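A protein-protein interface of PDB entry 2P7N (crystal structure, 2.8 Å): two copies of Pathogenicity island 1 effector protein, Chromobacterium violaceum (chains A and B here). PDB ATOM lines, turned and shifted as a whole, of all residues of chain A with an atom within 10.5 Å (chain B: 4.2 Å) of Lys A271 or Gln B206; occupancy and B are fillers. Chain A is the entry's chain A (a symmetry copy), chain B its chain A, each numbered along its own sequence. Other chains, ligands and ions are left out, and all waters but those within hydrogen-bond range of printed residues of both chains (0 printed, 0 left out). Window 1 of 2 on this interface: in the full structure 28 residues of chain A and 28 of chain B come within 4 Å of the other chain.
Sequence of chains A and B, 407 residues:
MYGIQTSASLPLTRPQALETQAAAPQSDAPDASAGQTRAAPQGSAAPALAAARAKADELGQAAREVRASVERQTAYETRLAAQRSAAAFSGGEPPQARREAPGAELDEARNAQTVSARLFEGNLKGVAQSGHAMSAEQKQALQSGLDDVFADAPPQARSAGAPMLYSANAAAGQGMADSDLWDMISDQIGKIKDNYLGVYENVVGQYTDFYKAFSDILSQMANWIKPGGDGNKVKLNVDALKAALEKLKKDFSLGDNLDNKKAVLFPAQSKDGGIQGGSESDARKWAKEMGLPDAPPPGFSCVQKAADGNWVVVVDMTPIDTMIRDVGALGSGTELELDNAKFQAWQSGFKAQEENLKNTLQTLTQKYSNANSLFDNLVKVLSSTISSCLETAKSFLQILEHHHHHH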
ATOM      1  N   LEU A 106      18.963  24.135  -9.585  1.00  0.00           N
ATOM      2  CA  LEU A 106      19.363  23.715  -8.266  1.00  0.00           C
ATOM      3  C   LEU A 106      20.212  24.614  -7.429  1.00  0.00           C
ATOM      4  O   LEU A 106      19.971  24.813  -6.259  1.00  0.00           O
ATOM      5  CB  LEU A 106      20.093  22.336  -8.341  1.00  0.00           C
ATOM      6  CG  LEU A 106      19.354  21.099  -8.883  1.00  0.00           C
ATOM      7  CD1 LEU A 106      20.144  19.837  -8.597  1.00  0.00           C
ATOM      8  CD2 LEU A 106      17.983  21.027  -8.247  1.00  0.00           C
ATOM      9  N   ASN A 202      10.169  18.748  -7.389  1.00  0.00           N
ATOM     10  CA  ASN A 202      10.842  17.476  -7.594  1.00  0.00           C
ATOM     11  C   ASN A 202      10.417  16.887  -8.929  1.00  0.00           C
ATOM     12  O   ASN A 202      11.258  16.449  -9.716  1.00  0.00           O
ATOM     13  CB  ASN A 202      10.508  16.495  -6.475  1.00  0.00           C
ATOM     14  CG  ASN A 202      10.992  15.085  -6.779  1.00  0.00           C
ATOM     15  OD1 ASN A 202      12.035  14.899  -7.406  1.00  0.00           O
ATOM     16  ND2 ASN A 202      10.244  14.089  -6.322  1.00  0.00           N
ATOM     17  N   GLN A 206      13.076  16.013 -11.679  1.00  0.00           N
ATOM     18  CA  GLN A 206      13.207  14.631 -12.123  1.00  0.00           C
ATOM     19  C   GLN A 206      12.898  14.483 -13.597  1.00  0.00           C
ATOM     20  O   GLN A 206      13.547  13.721 -14.304  1.00  0.00           O
ATOM     21  CB  GLN A 206      12.273  13.730 -11.315  1.00  0.00           C
ATOM     22  CG  GLN A 206      12.739  13.473  -9.890  1.00  0.00           C
ATOM     23  CD  GLN A 206      13.887  12.496  -9.829  1.00  0.00           C
ATOM     24  OE1 GLN A 206      14.786  12.529 -10.666  1.00  0.00           O
ATOM     25  NE2 GLN A 206      13.867  11.624  -8.832  1.00  0.00           N
ATOM     26  N   ASP A 259      13.675  -0.733  -8.199  1.00  0.00           N
ATOM     27  CA  ASP A 259      14.441   0.084  -7.263  1.00  0.00           C
ATOM     28  C   ASP A 259      15.051   1.363  -7.831  1.00  0.00           C
ATOM     29  O   ASP A 259      15.641   2.139  -7.084  1.00  0.00           O
ATOM     30  CB  ASP A 259      15.550  -0.761  -6.622  1.00  0.00           C
ATOM     31  CG  ASP A 259      16.783  -0.889  -7.509  1.00  0.00           C
ATOM     32  OD1 ASP A 259      17.449   0.143  -7.752  1.00  0.00           O
ATOM     33  OD2 ASP A 259      17.092  -2.016  -7.956  1.00  0.00           O
ATOM     34  N   ASN A 260      14.926   1.589  -9.136  1.00  0.00           N
ATOM     35  CA  ASN A 260      15.488   2.797  -9.737  1.00  0.00           C
ATOM     36  C   ASN A 260      14.661   4.026  -9.368  1.00  0.00           C
ATOM     37  O   ASN A 260      13.483   4.124  -9.708  1.00  0.00           O
ATOM     38  CB  ASN A 260      15.569   2.652 -11.255  1.00  0.00           C
ATOM     39  CG  ASN A 260      16.132   3.892 -11.927  1.00  0.00           C
ATOM     40  OD1 ASN A 260      17.124   4.467 -11.474  1.00  0.00           O
ATOM     41  ND2 ASN A 260      15.499   4.309 -13.023  1.00  0.00           N
ATOM     42  N   LYS A 261      15.296   4.966  -8.674  1.00  0.00           N
ATOM     43  CA  LYS A 261      14.637   6.188  -8.215  1.00  0.00           C
ATOM     44  C   LYS A 261      14.634   7.303  -9.258  1.00  0.00           C
ATOM     45  O   LYS A 261      13.804   8.210  -9.199  1.00  0.00           O
ATOM     46  CB  LYS A 261      15.316   6.683  -6.938  1.00  0.00           C
ATOM     47  CG  LYS A 261      15.566   5.590  -5.908  1.00  0.00           C
ATOM     48  CD  LYS A 261      16.109   6.139  -4.597  1.00  0.00           C
ATOM     49  CE  LYS A 261      17.612   6.344  -4.640  1.00  0.00           C
ATOM     50  NZ  LYS A 261      18.346   5.053  -4.760  1.00  0.00           N
ATOM     51  N   LYS A 262      15.561   7.234 -10.212  1.00  0.00           N
ATOM     52  CA  LYS A 262      15.659   8.245 -11.262  1.00  0.00           C
ATOM     53  C   LYS A 262      14.376   8.348 -12.084  1.00  0.00           C
ATOM     54  O   LYS A 262      14.161   9.340 -12.779  1.00  0.00           O
ATOM     55  CB  LYS A 262      16.847   7.933 -12.180  1.00  0.00           C
ATOM     56  CG  LYS A 262      18.205   8.122 -11.521  1.00  0.00           C
ATOM     57  CD  LYS A 262      19.324   7.433 -12.292  1.00  0.00           C
ATOM     58  CE  LYS A 262      19.480   7.974 -13.702  1.00  0.00           C
ATOM     59  NZ  LYS A 262      20.509   7.200 -14.467  1.00  0.00           N
ATOM     60  N   PRO A 267       6.882  10.046  -4.811  1.00  0.00           N
ATOM     61  CA  PRO A 267       7.206  11.303  -4.130  1.00  0.00           C
ATOM     62  C   PRO A 267       8.696  11.606  -4.236  1.00  0.00           C
ATOM     63  O   PRO A 267       9.442  10.833  -4.843  1.00  0.00           O
ATOM     64  CB  PRO A 267       6.781  11.029  -2.699  1.00  0.00           C
ATOM     65  CG  PRO A 267       7.161   9.598  -2.535  1.00  0.00           C
ATOM     66  CD  PRO A 267       6.675   8.965  -3.831  1.00  0.00           C
ATOM     67  N   ALA A 268       9.126  12.724  -3.655  1.00  0.00           N
ATOM     68  CA  ALA A 268      10.535  13.083  -3.681  1.00  0.00           C
ATOM     69  C   ALA A 268      11.315  11.854  -3.213  1.00  0.00           C
ATOM     70  O   ALA A 268      10.873  11.138  -2.310  1.00  0.00           O
ATOM     71  CB  ALA A 268      10.802  14.253  -2.758  1.00  0.00           C
ATOM     72  N   GLN A 269      12.460  11.603  -3.836  1.00  0.00           N
ATOM     73  CA  GLN A 269      13.277  10.458  -3.495  1.00  0.00           C
ATOM     74  C   GLN A 269      14.579  10.839  -2.808  1.00  0.00           C
ATOM     75  O   GLN A 269      15.139  11.908  -3.053  1.00  0.00           O
ATOM     76  CB  GLN A 269      13.588   9.649  -4.755  1.00  0.00           C
ATOM     77  CG  GLN A 269      12.425   8.854  -5.293  1.00  0.00           C
ATOM     78  CD  GLN A 269      11.865   7.892  -4.267  1.00  0.00           C
ATOM     79  OE1 GLN A 269      12.569   7.011  -3.775  1.00  0.00           O
ATOM     80  NE2 GLN A 269      10.585   8.055  -3.937  1.00  0.00           N
ATOM     81  N   SER A 270      15.058   9.956  -1.940  1.00  0.00           N
ATOM     82  CA  SER A 270      16.325  10.179  -1.250  1.00  0.00           C
ATOM     83  C   SER A 270      17.405  10.185  -2.325  1.00  0.00           C
ATOM     84  O   SER A 270      17.110  10.028  -3.510  1.00  0.00           O
ATOM     85  CB  SER A 270      16.581   9.049  -0.249  1.00  0.00           C
ATOM     86  OG  SER A 270      17.941   8.995   0.130  1.00  0.00           O
ATOM     87  N   LYS A 271      18.650  10.381  -1.923  1.00  0.00           N
ATOM     88  CA  LYS A 271      19.752  10.363  -2.881  1.00  0.00           C
ATOM     89  C   LYS A 271      20.465   9.018  -2.845  1.00  0.00           C
ATOM     90  O   LYS A 271      20.733   8.422  -3.885  1.00  0.00           O
ATOM     91  CB  LYS A 271      20.768  11.463  -2.579  1.00  0.00           C
ATOM     92  CG  LYS A 271      22.184  11.043  -2.936  1.00  0.00           C
ATOM     93  CD  LYS A 271      22.981  12.116  -3.638  1.00  0.00           C
ATOM     94  CE  LYS A 271      24.197  11.486  -4.298  1.00  0.00           C
ATOM     95  NZ  LYS A 271      24.943  12.441  -5.163  1.00  0.00           N
ATOM     96  N   ASP A 272      20.774   8.556  -1.637  1.00  0.00           N
ATOM     97  CA  ASP A 272      21.451   7.284  -1.452  1.00  0.00           C
ATOM     98  C   ASP A 272      20.579   6.279  -0.715  1.00  0.00           C
ATOM     99  O   ASP A 272      21.006   5.160  -0.434  1.00  0.00           O
ATOM    100  CB  ASP A 272      22.757   7.483  -0.680  1.00  0.00           C
ATOM    101  CG  ASP A 272      23.848   8.092  -1.536  1.00  0.00           C
ATOM    102  OD1 ASP A 272      24.121   7.544  -2.631  1.00  0.00           O
ATOM    103  OD2 ASP A 272      24.438   9.114  -1.120  1.00  0.00           O
ATOM    104  N   GLY A 273      19.354   6.685  -0.402  1.00  0.00           N
ATOM    105  CA  GLY A 273      18.445   5.804   0.304  1.00  0.00           C
ATOM    106  C   GLY A 273      17.641   4.940  -0.641  1.00  0.00           C
ATOM    107  O   GLY A 273      17.724   5.096  -1.866  1.00  0.00           O
ATOM    108  N   GLY A 274      16.858   4.031  -0.073  1.00  0.00           N
ATOM    109  CA  GLY A 274      16.043   3.157  -0.891  1.00  0.00           C
ATOM    110  C   GLY A 274      14.833   3.860  -1.477  1.00  0.00           C
ATOM    111  O   GLY A 274      14.503   4.980  -1.085  1.00  0.00           O
ATOM    112  N   ILE A 275      14.189   3.209  -2.436  1.00  0.00           N
ATOM    113  CA  ILE A 275      12.991   3.751  -3.055  1.00  0.00           C
ATOM    114  C   ILE A 275      12.003   3.958  -1.908  1.00  0.00           C
ATOM    115  O   ILE A 275      12.187   3.407  -0.826  1.00  0.00           O
ATOM    116  CB  ILE A 275      12.412   2.746  -4.063  1.00  0.00           C
ATOM    117  CG1 ILE A 275      12.898   1.343  -3.694  1.00  0.00           C
ATOM    118  CG2 ILE A 275      12.827   3.109  -5.474  1.00  0.00           C
ATOM    119  CD1 ILE A 275      12.502   0.286  -4.659  1.00  0.00           C
ATOM    120  N   GLN A 276      10.962   4.747  -2.133  1.00  0.00           N
ATOM    121  CA  GLN A 276       9.988   4.993  -1.085  1.00  0.00           C
ATOM    122  C   GLN A 276       8.700   5.570  -1.641  1.00  0.00           C
ATOM    123  O   GLN A 276       8.554   6.782  -1.760  1.00  0.00           O
ATOM    124  CB  GLN A 276      10.577   5.947  -0.045  1.00  0.00           C
ATOM    125  CG  GLN A 276       9.561   6.472   0.961  1.00  0.00           C
ATOM    126  CD  GLN A 276      10.107   7.616   1.788  1.00  0.00           C
ATOM    127  OE1 GLN A 276      10.866   8.457   1.288  1.00  0.00           O
ATOM    128  NE2 GLN A 276       9.714   7.668   3.054  1.00  0.00           N
ATOM    129  N   LEU B 106      22.629   0.934  -2.702  1.00  0.00           N
ATOM    130  CA  LEU B 106      21.781   1.877  -2.019  1.00  0.00           C
ATOM    131  C   LEU B 106      20.578   1.390  -1.280  1.00  0.00           C
ATOM    132  O   LEU B 106      20.307   1.786  -0.168  1.00  0.00           O
ATOM    133  CB  LEU B 106      21.290   2.976  -3.015  1.00  0.00           C
ATOM    134  CG  LEU B 106      22.311   3.887  -3.724  1.00  0.00           C
ATOM    135  CD1 LEU B 106      21.609   5.046  -4.405  1.00  0.00           C
ATOM    136  CD2 LEU B 106      23.310   4.391  -2.707  1.00  0.00           C
ATOM    137  N   ASN B 202      30.316   7.611   0.039  1.00  0.00           N
ATOM    138  CA  ASN B 202      29.919   8.561  -0.987  1.00  0.00           C
ATOM    139  C   ASN B 202      30.903   8.500  -2.143  1.00  0.00           C
ATOM    140  O   ASN B 202      30.499   8.428  -3.305  1.00  0.00           O
ATOM    141  CB  ASN B 202      29.877   9.981  -0.429  1.00  0.00           C
ATOM    142  CG  ASN B 202      29.706  11.025  -1.520  1.00  0.00           C
ATOM    143  OD1 ASN B 202      29.028  10.787  -2.520  1.00  0.00           O
ATOM    144  ND2 ASN B 202      30.308  12.192  -1.326  1.00  0.00           N
ATOM    145  N   VAL B 203      32.194   8.517  -1.814  1.00  0.00           N
ATOM    146  CA  VAL B 203      33.248   8.439  -2.817  1.00  0.00           C
ATOM    147  C   VAL B 203      33.009   7.296  -3.789  1.00  0.00           C
ATOM    148  O   VAL B 203      32.993   7.496  -4.998  1.00  0.00           O
ATOM    149  CB  VAL B 203      34.632   8.262  -2.148  1.00  0.00           C
ATOM    150  CG1 VAL B 203      35.619   7.639  -3.124  1.00  0.00           C
ATOM    151  CG2 VAL B 203      35.164   9.620  -1.691  1.00  0.00           C
ATOM    152  N   VAL B 204      32.821   6.095  -3.252  1.00  0.00           N
ATOM    153  CA  VAL B 204      32.587   4.909  -4.079  1.00  0.00           C
ATOM    154  C   VAL B 204      31.271   5.007  -4.841  1.00  0.00           C
ATOM    155  O   VAL B 204      31.204   4.647  -6.022  1.00  0.00           O
ATOM    156  CB  VAL B 204      32.585   3.621  -3.228  1.00  0.00           C
ATOM    157  CG1 VAL B 204      31.732   2.556  -3.884  1.00  0.00           C
ATOM    158  CG2 VAL B 204      34.017   3.119  -3.068  1.00  0.00           C
ATOM    159  N   GLY B 205      30.225   5.487  -4.166  1.00  0.00           N
ATOM    160  CA  GLY B 205      28.938   5.616  -4.823  1.00  0.00           C
ATOM    161  C   GLY B 205      29.072   6.541  -6.015  1.00  0.00           C
ATOM    162  O   GLY B 205      28.648   6.206  -7.127  1.00  0.00           O
ATOM    163  N   GLN B 206      29.678   7.704  -5.784  1.00  0.00           N
ATOM    164  CA  GLN B 206      29.881   8.696  -6.832  1.00  0.00           C
ATOM    165  C   GLN B 206      30.769   8.170  -7.939  1.00  0.00           C
ATOM    166  O   GLN B 206      30.542   8.441  -9.113  1.00  0.00           O
ATOM    167  CB  GLN B 206      30.502   9.962  -6.242  1.00  0.00           C
ATOM    168  CG  GLN B 206      29.533  10.804  -5.426  1.00  0.00           C
ATOM    169  CD  GLN B 206      28.566  11.570  -6.295  1.00  0.00           C
ATOM    170  OE1 GLN B 206      28.080  11.057  -7.300  1.00  0.00           O
ATOM    171  NE2 GLN B 206      28.276  12.804  -5.908  1.00  0.00           N
ATOM    172  N   TYR B 207      31.784   7.407  -7.565  1.00  0.00           N
ATOM    173  CA  TYR B 207      32.700   6.872  -8.561  1.00  0.00           C
ATOM    174  C   TYR B 207      32.059   5.757  -9.380  1.00  0.00           C
ATOM    175  O   TYR B 207      32.337   5.620 -10.578  1.00  0.00           O
ATOM    176  CB  TYR B 207      33.983   6.338  -7.913  1.00  0.00           C
ATOM    177  CG  TYR B 207      35.059   6.162  -8.936  1.00  0.00           C
ATOM    178  CD1 TYR B 207      35.866   7.234  -9.309  1.00  0.00           C
ATOM    179  CD2 TYR B 207      35.201   4.962  -9.625  1.00  0.00           C
ATOM    180  CE1 TYR B 207      36.783   7.121 -10.356  1.00  0.00           C
ATOM    181  CE2 TYR B 207      36.113   4.838 -10.676  1.00  0.00           C
ATOM    182  CZ  TYR B 207      36.894   5.923 -11.033  1.00  0.00           C
ATOM    183  OH  TYR B 207      37.762   5.816 -12.093  1.00  0.00           O
ATOM    184  N   THR B 208      31.207   4.963  -8.738  1.00  0.00           N
ATOM    185  CA  THR B 208      30.537   3.859  -9.409  1.00  0.00           C
ATOM    186  C   THR B 208      29.539   4.334 -10.460  1.00  0.00           C
ATOM    187  O   THR B 208      29.271   3.625 -11.425  1.00  0.00           O
ATOM    188  CB  THR B 208      29.796   2.964  -8.402  1.00  0.00           C
ATOM    189  OG1 THR B 208      30.744   2.342  -7.528  1.00  0.00           O
ATOM    190  CG2 THR B 208      28.998   1.882  -9.127  1.00  0.00           C
ATOM    191  N   ASP B 209      28.971   5.523 -10.269  1.00  0.00           N
ATOM    192  CA  ASP B 209      28.022   6.056 -11.235  1.00  0.00           C
ATOM    193  C   ASP B 209      28.781   6.449 -12.494  1.00  0.00           C
ATOM    194  O   ASP B 209      28.289   6.291 -13.612  1.00  0.00           O
ATOM    195  CB  ASP B 209      27.285   7.263 -10.664  1.00  0.00           C
ATOM    196  CG  ASP B 209      26.282   6.877  -9.590  1.00  0.00           C
ATOM    197  OD1 ASP B 209      25.601   5.844  -9.765  1.00  0.00           O
ATOM    198  OD2 ASP B 209      26.161   7.609  -8.577  1.00  0.00           O
ATOM    199  N   PHE B 210      29.994   6.951 -12.295  1.00  0.00           N
ATOM    200  CA  PHE B 210      30.867   7.354 -13.388  1.00  0.00           C
ATOM    201  C   PHE B 210      31.285   6.113 -14.160  1.00  0.00           C
ATOM    202  O   PHE B 210      31.204   6.061 -15.387  1.00  0.00           O
ATOM    203  CB  PHE B 210      32.105   8.051 -12.827  1.00  0.00           C
ATOM    204  CG  PHE B 210      33.228   8.192 -13.819  1.00  0.00           C
ATOM    205  CD1 PHE B 210      33.086   8.986 -14.948  1.00  0.00           C
ATOM    206  CD2 PHE B 210      34.434   7.528 -13.616  1.00  0.00           C
ATOM    207  CE1 PHE B 210      34.125   9.118 -15.859  1.00  0.00           C
ATOM    208  CE2 PHE B 210      35.481   7.653 -14.521  1.00  0.00           C
ATOM    209  CZ  PHE B 210      35.326   8.450 -15.646  1.00  0.00           C
ATOM    210  N   LYS B 261      27.609  18.574  -9.466  1.00  0.00           N
ATOM    211  CA  LYS B 261      27.898  17.784  -8.270  1.00  0.00           C
ATOM    212  C   LYS B 261      28.202  16.318  -8.570  1.00  0.00           C
ATOM    213  O   LYS B 261      28.838  15.636  -7.767  1.00  0.00           O
ATOM    214  CB  LYS B 261      26.715  17.875  -7.305  1.00  0.00           C
ATOM    215  CG  LYS B 261      26.189  19.290  -7.104  1.00  0.00           C
ATOM    216  CD  LYS B 261      25.111  19.363  -6.032  1.00  0.00           C
ATOM    217  CE  LYS B 261      23.739  19.005  -6.573  1.00  0.00           C
ATOM    218  NZ  LYS B 261      23.255  20.006  -7.565  1.00  0.00           N
ATOM    219  N   LYS B 262      27.748  15.836  -9.726  1.00  0.00           N
ATOM    220  CA  LYS B 262      27.974  14.448 -10.121  1.00  0.00           C
ATOM    221  C   LYS B 262      29.460  14.109 -10.205  1.00  0.00           C
ATOM    222  O   LYS B 262      29.831  12.935 -10.204  1.00  0.00           O
ATOM    223  CB  LYS B 262      27.293  14.169 -11.466  1.00  0.00           C
ATOM    224  CG  LYS B 262      25.774  14.168 -11.403  1.00  0.00           C
ATOM    225  CD  LYS B 262      25.136  14.296 -12.781  1.00  0.00           C
ATOM    226  CE  LYS B 262      25.503  13.146 -13.702  1.00  0.00           C
ATOM    227  NZ  LYS B 262      24.955  13.361 -15.079  1.00  0.00           N
ATOM    228  N   VAL B 264      31.677  15.183  -7.935  1.00  0.00           N
ATOM    229  CA  VAL B 264      32.259  15.367  -6.618  1.00  0.00           C
ATOM    230  C   VAL B 264      32.439  14.097  -5.797  1.00  0.00           C
ATOM    231  O   VAL B 264      31.461  13.419  -5.445  1.00  0.00           O
ATOM    232  CB  VAL B 264      31.435  16.372  -5.790  1.00  0.00           C
ATOM    233  CG1 VAL B 264      31.983  16.459  -4.372  1.00  0.00           C
ATOM    234  CG2 VAL B 264      31.461  17.741  -6.462  1.00  0.00           C
ATOM    235  N   LEU B 265      33.698  13.788  -5.482  1.00  0.00           N
ATOM    236  CA  LEU B 265      34.035  12.620  -4.684  1.00  0.00           C
ATOM    237  C   LEU B 265      34.002  13.008  -3.213  1.00  0.00           C
ATOM    238  O   LEU B 265      33.733  12.184  -2.338  1.00  0.00           O
ATOM    239  CB  LEU B 265      35.425  12.113  -5.056  1.00  0.00           C
ATOM    240  CG  LEU B 265      35.570  11.548  -6.469  1.00  0.00           C
ATOM    241  CD1 LEU B 265      37.016  11.147  -6.720  1.00  0.00           C
ATOM    242  CD2 LEU B 265      34.643  10.343  -6.640  1.00  0.00           C
ATOM    243  N   GLN B 269      27.555  15.303  -1.417  1.00  0.00           N
ATOM    244  CA  GLN B 269      26.794  16.383  -2.011  1.00  0.00           C
ATOM    245  C   GLN B 269      25.294  16.232  -1.814  1.00  0.00           C
ATOM    246  O   GLN B 269      24.771  15.120  -1.732  1.00  0.00           O
ATOM    247  CB  GLN B 269      27.101  16.472  -3.506  1.00  0.00           C
ATOM    248  CG  GLN B 269      28.459  17.040  -3.835  1.00  0.00           C
ATOM    249  CD  GLN B 269      28.658  18.423  -3.251  1.00  0.00           C
ATOM    250  OE1 GLN B 269      27.912  19.352  -3.557  1.00  0.00           O
ATOM    251  NE2 GLN B 269      29.673  18.568  -2.402  1.00  0.00           N
ATOM    252  N   LYS B 271      21.282  16.622  -2.963  1.00  0.00           N
ATOM    253  CA  LYS B 271      20.665  16.074  -4.168  1.00  0.00           C
ATOM    254  C   LYS B 271      20.144  17.198  -5.053  1.00  0.00           C
ATOM    255  O   LYS B 271      20.379  17.207  -6.259  1.00  0.00           O
ATOM    256  CB  LYS B 271      19.504  15.143  -3.824  1.00  0.00           C
ATOM    257  CG  LYS B 271      18.403  15.197  -4.869  1.00  0.00           C
ATOM    258  CD  LYS B 271      17.847  13.843  -5.241  1.00  0.00           C
ATOM    259  CE  LYS B 271      17.071  13.961  -6.543  1.00  0.00           C
ATOM    260  NZ  LYS B 271      16.639  12.641  -7.077  1.00  0.00           N
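The backbone carbonyl oxygen (O) of Pro A267 is in hydrogen-bond range of the side-chain amide nitrogen (NE2) of Gln A269.
The side-chain amide nitrogen (NE2) of Gln B206 sits close to the backbone carbonyl oxygen (O) of Val B264 (3.3 Å).
NZ of Lys A261 is in hydrogen-bond range of O of Gly A273 (3.0 Å).
The backbone carbonyl oxygen (O) of Lys B261 lies within hydrogen-bond range of the side-chain amide nitrogen (NE2) of Gln B206, at 3.4 Å.
N of Gln A276 is in hydrogen-bond range of OE1 of Gln A269.
OG of Ser A270 sits at hydrogen-bond distance from N of Asp A272 (3.4 Å).
The side-chain amino group of Lys B271 lies close to the side-chain amide nitrogen of Gln A206 (3.4 Å).
O of Asp A272 lies close to O of Leu B106.
The side-chain amide nitrogen (NE2) of Gln B206 lies close to the side-chain amino group (NZ) of Lys A271 (3.4 Å).
Of the printed residues of chain B, Lys A271 touches Leu B106, Gln B206 and Gln B269.
Gln B206 touches just one residue of chain A: Lys A271.
No residue of chain A comes within 4 Å of Asn B202.
Asp B209 touches none of the printed residues of chain A.
No residue of chain A comes within 4 Å of Val B264.
Of the printed residues of chain A, Lys B271 touches Leu A106, Gln A206 and Gln A269.
Of the printed residues of chain B, Asp A272 touches Leu B106.
Printed residues of chain A within 4 Å of Gln B269: Lys A271.
Gln A276 touches none of the printed residues of chain B.
The nearest printed residue of chain B that does not touch Lys A271 is Lys B271 (4.1 Å).
The nearest residue of chain A that does not touch Gln B206 is Asp A272 (6.4 Å).
The nearest printed residue of chain A that does not touch Gln B269 is Asp A272 (6.0 Å).
Leu A106 touches Lys B261, and with the chains exchanged Lys A261 touches Leu B106.
Leu A106 touches Lys B271, and with the chains exchanged Lys A271 touches Leu B106.
Gln A206 touches Lys B271, and with the chains exchanged Lys A271 touches Gln B206.
Gln A269 touches Lys B271, and with the chains exchanged Lys A271 touches Gln B269.
Of the 9 pairs that touch across the chains among the printed residues, 8 have their exchanged pair printed and touching as well.
Of the 16 printed residues of chain B, 5 touch a printed residue of chain A.
Printed residues of chain B that touch a printed residue of chain A: Leu B106, Gln B206, Lys B261, Gln B269 and Lys B271.
Hydrophobic or aromatic side chains of chain B that line the printed part of chain A: Leu B106.
Printed residues of chain A that touch a printed residue of chain B: Leu A106, Gln A206, Lys A261, Gln A269, Lys A271 and Asp A272.
Among the printed residues, 9 pairs touch across the chains.
Among the printed residues, no Asp or Glu carboxylate lies within 4 Å of a Lys or Arg side-chain nitrogen of the other chain.
Among the printed residues, merely in contact across the chains: Leu A106 with Lys B261, Leu A106 with Lys B271, Lys A261 with Leu B106, Gln A269 with Lys B271, Lys A271 with Leu B106 and Lys A271 with Gln B269.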
